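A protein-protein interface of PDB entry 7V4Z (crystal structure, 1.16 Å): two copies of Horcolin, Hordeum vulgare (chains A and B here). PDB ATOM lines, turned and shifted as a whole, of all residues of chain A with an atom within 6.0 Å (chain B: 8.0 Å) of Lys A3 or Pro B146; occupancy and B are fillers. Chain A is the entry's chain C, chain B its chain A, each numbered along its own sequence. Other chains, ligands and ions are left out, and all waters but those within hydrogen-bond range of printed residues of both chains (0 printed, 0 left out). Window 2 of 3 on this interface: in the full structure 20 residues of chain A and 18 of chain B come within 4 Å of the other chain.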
ATOM      1  N   LYS A   3       2.731  -5.485   8.942  1.00  0.00           N
ATOM      2  CA  LYS A   3       1.266  -5.568   8.616  1.00  0.00           C
ATOM      3  C   LYS A   3       1.067  -6.081   7.193  1.00  0.00           C
ATOM      4  O   LYS A   3       1.711  -5.561   6.263  1.00  0.00           O
ATOM      5  CB  LYS A   3       0.601  -4.210   8.721  1.00  0.00           C
ATOM      6  N   PRO A   4       0.211  -7.085   6.976  1.00  0.00           N
ATOM      7  CA  PRO A   4       0.086  -7.606   5.645  1.00  0.00           C
ATOM      8  C   PRO A   4      -0.764  -6.718   4.755  1.00  0.00           C
ATOM      9  O   PRO A   4      -1.680  -6.072   5.186  1.00  0.00           O
ATOM     10  CB  PRO A   4      -0.526  -8.964   5.817  1.00  0.00           C
ATOM     11  CG  PRO A   4      -1.402  -8.784   6.989  1.00  0.00           C
ATOM     12  CD  PRO A   4      -0.529  -7.941   7.897  1.00  0.00           C
ATOM     13  N   VAL A   5      -0.467  -6.778   3.472  1.00  0.00           N
ATOM     14  CA  VAL A   5      -1.424  -6.369   2.420  1.00  0.00           C
ATOM     15  C   VAL A   5      -2.443  -7.455   2.231  1.00  0.00           C
ATOM     16  O   VAL A   5      -2.091  -8.632   2.331  1.00  0.00           O
ATOM     17  CB  VAL A   5      -0.626  -6.011   1.175  1.00  0.00           C
ATOM     18  CG1 VAL A   5      -1.357  -6.108  -0.107  1.00  0.00           C
ATOM     19  CG2 VAL A   5       0.279  -4.846   1.317  1.00  0.00           C
ATOM     20  N   PRO A  24      -2.284 -12.387   9.474  1.00  0.00           N
ATOM     21  CA  PRO A  24      -1.015 -13.110   9.419  1.00  0.00           C
ATOM     22  C   PRO A  24       0.145 -12.291   8.871  1.00  0.00           C
ATOM     23  O   PRO A  24      -0.044 -11.536   7.907  1.00  0.00           O
ATOM     24  CB  PRO A  24      -1.343 -14.257   8.492  1.00  0.00           C
ATOM     25  CG  PRO A  24      -2.327 -13.656   7.560  1.00  0.00           C
ATOM     26  CD  PRO A  24      -3.179 -12.723   8.357  1.00  0.00           C
ATOM     27  N   ILE A  25       1.325 -12.500   9.420  1.00  0.00           N
ATOM     28  CA  ILE A  25       2.578 -11.928   8.861  1.00  0.00           C
ATOM     29  C   ILE A  25       3.481 -12.989   8.272  1.00  0.00           C
ATOM     30  O   ILE A  25       4.330 -12.634   7.412  1.00  0.00           O
ATOM     31  CB  ILE A  25       3.337 -11.055   9.858  1.00  0.00           C
ATOM     32  CG1 ILE A  25       3.914 -11.878  11.011  1.00  0.00           C
ATOM     33  CG2 ILE A  25       2.457  -9.878  10.313  1.00  0.00           C
ATOM     34  CD1 ILE A  25       4.738 -11.044  11.979  1.00  0.00           C
ATOM     35  N   THR A  48       0.176 -10.683  13.510  1.00  0.00           N
ATOM     36  CA  THR A  48       0.770  -9.341  13.730  1.00  0.00           C
ATOM     37  C   THR A  48       1.254  -9.189  15.169  1.00  0.00           C
ATOM     38  O   THR A  48       2.034  -8.272  15.447  1.00  0.00           O
ATOM     39  CB  THR A  48      -0.251  -8.258  13.351  1.00  0.00           C
ATOM     40  OG1 THR A  48      -1.454  -8.540  14.062  1.00  0.00           O
ATOM     41  CG2 THR A  48      -0.508  -8.195  11.877  1.00  0.00           C
ATOM     42  N   ILE A 144      -0.176 -10.776   2.214  1.00  0.00           N
ATOM     43  CA  ILE A 144       1.207 -10.788   1.669  1.00  0.00           C
ATOM     44  C   ILE A 144       2.041  -9.855   2.528  1.00  0.00           C
ATOM     45  O   ILE A 144       1.621  -8.703   2.831  1.00  0.00           O
ATOM     46  CB  ILE A 144       1.218 -10.333   0.214  1.00  0.00           C
ATOM     47  CG1 ILE A 144       0.198 -11.141  -0.624  1.00  0.00           C
ATOM     48  CG2 ILE A 144       2.626 -10.455  -0.384  1.00  0.00           C
ATOM     49  CD1 ILE A 144       0.155 -10.773  -2.067  1.00  0.00           C
ATOM     50  N   THR A 145       3.231 -10.283   2.905  1.00  0.00           N
ATOM     51  CA  THR A 145       4.202  -9.423   3.611  1.00  0.00           C
ATOM     52  C   THR A 145       5.471  -9.329   2.803  1.00  0.00           C
ATOM     53  O   THR A 145       5.830 -10.238   2.075  1.00  0.00           O
ATOM     54  CB  THR A 145       4.483  -9.855   5.047  1.00  0.00           C
ATOM     55  OG1 THR A 145       4.837 -11.240   4.948  1.00  0.00           O
ATOM     56  CG2 THR A 145       3.275  -9.619   5.925  1.00  0.00           C
ATOM     57  N   PRO A 146       6.162  -8.169   2.875  1.00  0.00           N
ATOM     58  CA  PRO A 146       7.430  -7.991   2.187  1.00  0.00           C
ATOM     59  C   PRO A 146       8.572  -8.747   2.894  1.00  0.00           C
ATOM     60  O   PRO A 146       9.625  -8.738   2.178  1.00  0.00           O
ATOM     61  CB  PRO A 146       7.587  -6.464   2.201  1.00  0.00           C
ATOM     62  CG  PRO A 146       6.962  -6.056   3.472  1.00  0.00           C
ATOM     63  CD  PRO A 146       5.815  -6.999   3.696  1.00  0.00           C
ATOM     64  N   LYS B   3       9.303  -1.062   2.506  1.00  0.00           N
ATOM     65  CA  LYS B   3       7.974  -1.352   3.126  1.00  0.00           C
ATOM     66  C   LYS B   3       7.000  -1.873   2.076  1.00  0.00           C
ATOM     67  O   LYS B   3       6.103  -2.569   2.531  1.00  0.00           O
ATOM     68  CB  LYS B   3       7.382  -0.179   3.903  1.00  0.00           C
ATOM     69  N   PRO B   4       6.919  -1.462   0.769  1.00  0.00           N
ATOM     70  CA  PRO B   4       5.869  -2.040  -0.066  1.00  0.00           C
ATOM     71  C   PRO B   4       6.169  -3.487  -0.413  1.00  0.00           C
ATOM     72  O   PRO B   4       7.276  -3.917  -0.505  1.00  0.00           O
ATOM     73  CB  PRO B   4       5.853  -1.150  -1.313  1.00  0.00           C
ATOM     74  CG  PRO B   4       7.254  -0.772  -1.465  1.00  0.00           C
ATOM     75  CD  PRO B   4       7.673  -0.464  -0.040  1.00  0.00           C
ATOM     76  N   VAL B   5       5.098  -4.226  -0.627  1.00  0.00           N
ATOM     77  CA  VAL B   5       5.165  -5.543  -1.288  1.00  0.00           C
ATOM     78  C   VAL B   5       5.258  -5.296  -2.780  1.00  0.00           C
ATOM     79  O   VAL B   5       4.716  -4.309  -3.291  1.00  0.00           O
ATOM     80  CB  VAL B   5       3.998  -6.433  -0.906  1.00  0.00           C
ATOM     81  CG1 VAL B   5       3.826  -6.657   0.568  1.00  0.00           C
ATOM     82  CG2 VAL B   5       2.750  -6.248  -1.541  1.00  0.00           C
ATOM     83  N   ILE B  25       6.416   4.564  -1.618  1.00  0.00           N
ATOM     84  CA  ILE B  25       5.478   4.333  -0.482  1.00  0.00           C
ATOM     85  C   ILE B  25       4.148   5.010  -0.737  1.00  0.00           C
ATOM     86  O   ILE B  25       3.249   4.878   0.092  1.00  0.00           O
ATOM     87  CB  ILE B  25       6.087   4.820   0.850  1.00  0.00           C
ATOM     88  CG1 ILE B  25       6.236   6.351   0.935  1.00  0.00           C
ATOM     89  CG2 ILE B  25       7.387   4.102   1.153  1.00  0.00           C
ATOM     90  CD1 ILE B  25       6.727   6.856   2.265  1.00  0.00           C
ATOM     91  N   VAL B 120      -7.204  -4.379  -3.881  1.00  0.00           N
ATOM     92  CA  VAL B 120      -6.484  -4.189  -2.606  1.00  0.00           C
ATOM     93  C   VAL B 120      -7.505  -3.763  -1.578  1.00  0.00           C
ATOM     94  O   VAL B 120      -8.306  -2.804  -1.810  1.00  0.00           O
ATOM     95  CB  VAL B 120      -5.374  -3.160  -2.754  1.00  0.00           C
ATOM     96  CG1 VAL B 120      -4.577  -3.139  -1.473  1.00  0.00           C
ATOM     97  CG2 VAL B 120      -4.488  -3.492  -3.919  1.00  0.00           C
ATOM     98  N   LEU B 121      -7.515  -4.447  -0.458  1.00  0.00           N
ATOM     99  CA  LEU B 121      -8.558  -4.288   0.549  1.00  0.00           C
ATOM    100  C   LEU B 121      -7.987  -3.606   1.806  1.00  0.00           C
ATOM    101  O   LEU B 121      -6.772  -3.462   1.988  1.00  0.00           O
ATOM    102  CB  LEU B 121      -9.124  -5.660   0.922  1.00  0.00           C
ATOM    103  CG  LEU B 121      -9.666  -6.500  -0.227  1.00  0.00           C
ATOM    104  CD1 LEU B 121     -10.214  -7.826   0.260  1.00  0.00           C
ATOM    105  CD2 LEU B 121     -10.706  -5.790  -1.079  1.00  0.00           C
ATOM    106  N   ASP B 122      -8.909  -3.199   2.679  1.00  0.00           N
ATOM    107  CA  ASP B 122      -8.558  -2.799   4.047  1.00  0.00           C
ATOM    108  C   ASP B 122      -7.635  -1.593   4.122  1.00  0.00           C
ATOM    109  O   ASP B 122      -6.916  -1.441   5.086  1.00  0.00           O
ATOM    110  CB  ASP B 122      -8.003  -3.970   4.868  1.00  0.00           C
ATOM    111  CG  ASP B 122      -9.048  -5.009   5.207  1.00  0.00           C
ATOM    112  OD1 ASP B 122     -10.278  -4.791   4.900  1.00  0.00           O
ATOM    113  OD2 ASP B 122      -8.666  -5.987   5.925  1.00  0.00           O
ATOM    114  N   GLY B 123      -7.778  -0.674   3.180  1.00  0.00           N
ATOM    115  CA  GLY B 123      -6.996   0.569   3.146  1.00  0.00           C
ATOM    116  C   GLY B 123      -5.635   0.394   2.583  1.00  0.00           C
ATOM    117  O   GLY B 123      -4.895   1.399   2.500  1.00  0.00           O
ATOM    118  N   GLY B 124      -5.251  -0.764   2.050  1.00  0.00           N
ATOM    119  CA  GLY B 124      -4.031  -0.878   1.260  1.00  0.00           C
ATOM    120  C   GLY B 124      -4.141  -0.113  -0.048  1.00  0.00           C
ATOM    121  O   GLY B 124      -5.243   0.170  -0.519  1.00  0.00           O
ATOM    122  N   LYS B 125      -3.009   0.141  -0.674  1.00  0.00           N
ATOM    123  CA  LYS B 125      -2.974   1.104  -1.805  1.00  0.00           C
ATOM    124  C   LYS B 125      -1.921   0.689  -2.808  1.00  0.00           C
ATOM    125  O   LYS B 125      -0.839   0.215  -2.392  1.00  0.00           O
ATOM    126  CB  LYS B 125      -2.642   2.526  -1.291  1.00  0.00           C
ATOM    127  CG  LYS B 125      -3.237   2.958   0.032  1.00  0.00           C
ATOM    128  CD  LYS B 125      -2.796   4.346   0.454  1.00  0.00           C
ATOM    129  CE  LYS B 125      -3.485   4.835   1.704  1.00  0.00           C
ATOM    130  NZ  LYS B 125      -3.437   3.839   2.774  1.00  0.00           N
ATOM    131  N   ILE B 126      -2.184   0.847  -4.081  1.00  0.00           N
ATOM    132  CA  ILE B 126      -1.116   0.722  -5.096  1.00  0.00           C
ATOM    133  C   ILE B 126      -0.249   1.926  -5.057  1.00  0.00           C
ATOM    134  O   ILE B 126      -0.781   3.061  -5.286  1.00  0.00           O
ATOM    135  CB  ILE B 126      -1.707   0.382  -6.483  1.00  0.00           C
ATOM    136  CG1 ILE B 126      -2.339  -1.050  -6.377  1.00  0.00           C
ATOM    137  CG2 ILE B 126      -0.571   0.404  -7.513  1.00  0.00           C
ATOM    138  CD1 ILE B 126      -3.071  -1.630  -7.540  1.00  0.00           C
ATOM    139  N   ALA B 127       1.008   1.767  -4.711  1.00  0.00           N
ATOM    140  CA  ALA B 127       1.972   2.876  -4.527  1.00  0.00           C
ATOM    141  C   ALA B 127       2.839   3.144  -5.740  1.00  0.00           C
ATOM    142  O   ALA B 127       3.512   4.186  -5.778  1.00  0.00           O
ATOM    143  CB  ALA B 127       2.868   2.575  -3.352  1.00  0.00           C
ATOM    144  N   TYR B 143       3.665  -2.185  -6.752  1.00  0.00           N
ATOM    145  CA  TYR B 143       4.090  -1.988  -5.382  1.00  0.00           C
ATOM    146  C   TYR B 143       2.850  -1.639  -4.578  1.00  0.00           C
ATOM    147  O   TYR B 143       2.074  -0.786  -5.006  1.00  0.00           O
ATOM    148  CB  TYR B 143       5.100  -0.849  -5.299  1.00  0.00           C
ATOM    149  CG  TYR B 143       6.448  -1.208  -5.889  1.00  0.00           C
ATOM    150  CD1 TYR B 143       7.333  -1.981  -5.178  1.00  0.00           C
ATOM    151  CD2 TYR B 143       6.861  -0.729  -7.123  1.00  0.00           C
ATOM    152  CE1 TYR B 143       8.576  -2.319  -5.693  1.00  0.00           C
ATOM    153  CE2 TYR B 143       8.085  -1.061  -7.648  1.00  0.00           C
ATOM    154  CZ  TYR B 143       8.966  -1.854  -6.923  1.00  0.00           C
ATOM    155  OH  TYR B 143      10.202  -2.238  -7.371  1.00  0.00           O
ATOM    156  N   ILE B 144       2.670  -2.292  -3.441  1.00  0.00           N
ATOM    157  CA  ILE B 144       1.427  -2.141  -2.642  1.00  0.00           C
ATOM    158  C   ILE B 144       1.834  -1.910  -1.196  1.00  0.00           C
ATOM    159  O   ILE B 144       2.624  -2.688  -0.658  1.00  0.00           O
ATOM    160  CB  ILE B 144       0.506  -3.355  -2.807  1.00  0.00           C
ATOM    161  CG1 ILE B 144       0.301  -3.693  -4.264  1.00  0.00           C
ATOM    162  CG2 ILE B 144      -0.819  -3.122  -2.077  1.00  0.00           C
ATOM    163  CD1 ILE B 144      -0.627  -4.840  -4.527  1.00  0.00           C
ATOM    164  N   THR B 145       1.224  -0.925  -0.564  1.00  0.00           N
ATOM    165  CA  THR B 145       1.447  -0.662   0.871  1.00  0.00           C
ATOM    166  C   THR B 145       0.182  -1.017   1.628  1.00  0.00           C
ATOM    167  O   THR B 145      -0.932  -0.928   1.105  1.00  0.00           O
ATOM    168  CB  THR B 145       1.817   0.799   1.103  1.00  0.00           C
ATOM    169  OG1 THR B 145       0.767   1.632   0.578  1.00  0.00           O
ATOM    170  CG2 THR B 145       3.116   1.207   0.465  1.00  0.00           C
ATOM    171  N   PRO B 146       0.318  -1.532   2.845  1.00  0.00           N
ATOM    172  CA  PRO B 146      -0.842  -1.857   3.667  1.00  0.00           C
ATOM    173  C   PRO B 146      -1.440  -0.599   4.344  1.00  0.00           C
ATOM    174  O   PRO B 146      -2.613  -1.050   4.736  1.00  0.00           O
ATOM    175  CB  PRO B 146      -0.220  -2.850   4.662  1.00  0.00           C
ATOM    176  CG  PRO B 146       1.141  -2.349   4.897  1.00  0.00           C
ATOM    177  CD  PRO B 146       1.588  -1.871   3.525  1.00  0.00           C
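The backbone carbonyl oxygen (O) of Val B5 sits at hydrogen-bond distance from the backbone NH (N) of Ile B144, 2.9 Å away. N of Lys B125 is in hydrogen-bond range of O of Thr B145 (2.9 Å). O of Val A5 lies within hydrogen-bond range of N of Ile A144, at 2.9 Å. OG1 of Thr A145 lies within hydrogen-bond range of O of Ile A25, 2.9 Å away.
Among the printed residues, merely in contact across the chains: Lys A3 with Pro B146 (3.5 Å), Pro A4 with Pro B146 (3.6 Å), Pro A146 with Val B5 (3.6 Å), Val A5 with Ile B144 (3.6 Å), Val A5 with Pro B146 (3.6 Å), Pro A146 with Lys B3 (3.7 Å), Pro A146 with Pro B4 (3.7 Å), Ile A144 with Val B5 (3.8 Å), Val A5 with Thr B145 (3.8 Å) and Thr A145 with Val B5 (3.9 Å).
Of chain B, only Pro B146 comes within 4 Å of Lys A3. Pro A4 touches just one residue of chain B: Pro B146. Ile A25 touches none of the printed residues of chain B. Of the printed residues of chain B, Thr A145 touches Val B5 (3.9 Å). Of the printed residues of chain B, Pro A146 touches Lys B3 (3.7 Å), Pro B4 (3.7 Å) and Val B5 (3.6 Å). Printed residues of chain A within 4 Å of Lys B3: Pro A146 (3.7 Å). Printed residues of chain A within 4 Å of Pro B4: Pro A146 (3.7 Å). Of the printed residues of chain A, Ile B144 touches Val A5. The nearest printed residue of chain A that does not touch Pro B146 is Ile A144 (6.4 Å).
Of the 16 printed residues of chain B, 6 touch a printed residue of chain A. Hydrophobic or aromatic side chains of chain B that line the printed part of chain A: Val B5, Ile B144 and Pro B146. Of the 9 printed residues of chain A, 6 touch a printed residue of chain B. Printed residues of chain A that touch a printed residue of chain B: Lys A3, Pro A4, Val A5, Ile A144, Thr A145 and Pro A146. Among the printed residues, 10 pairs touch across the chains. Among the printed residues, no Asp or Glu carboxylate lies within 4 Å of a Lys or Arg side-chain nitrogen of the other chain.
Pro A4 touches Pro B146, and with the chains exchanged Pro A146 touches Pro B4. Val A5 touches Ile B144, and with the chains exchanged Ile A144 touches Val B5. Val A5 touches Thr B145, and with the chains exchanged Thr A145 touches Val B5. Val A5 touches Pro B146, and with the chains exchanged Pro A146 touches Val B5. Positions printed for both chains: 3, 4, 5, 25, 144, 145 and 146. Of the 10 pairs that touch across the chains among the printed residues, 10 have their exchanged pair printed and touching as well.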
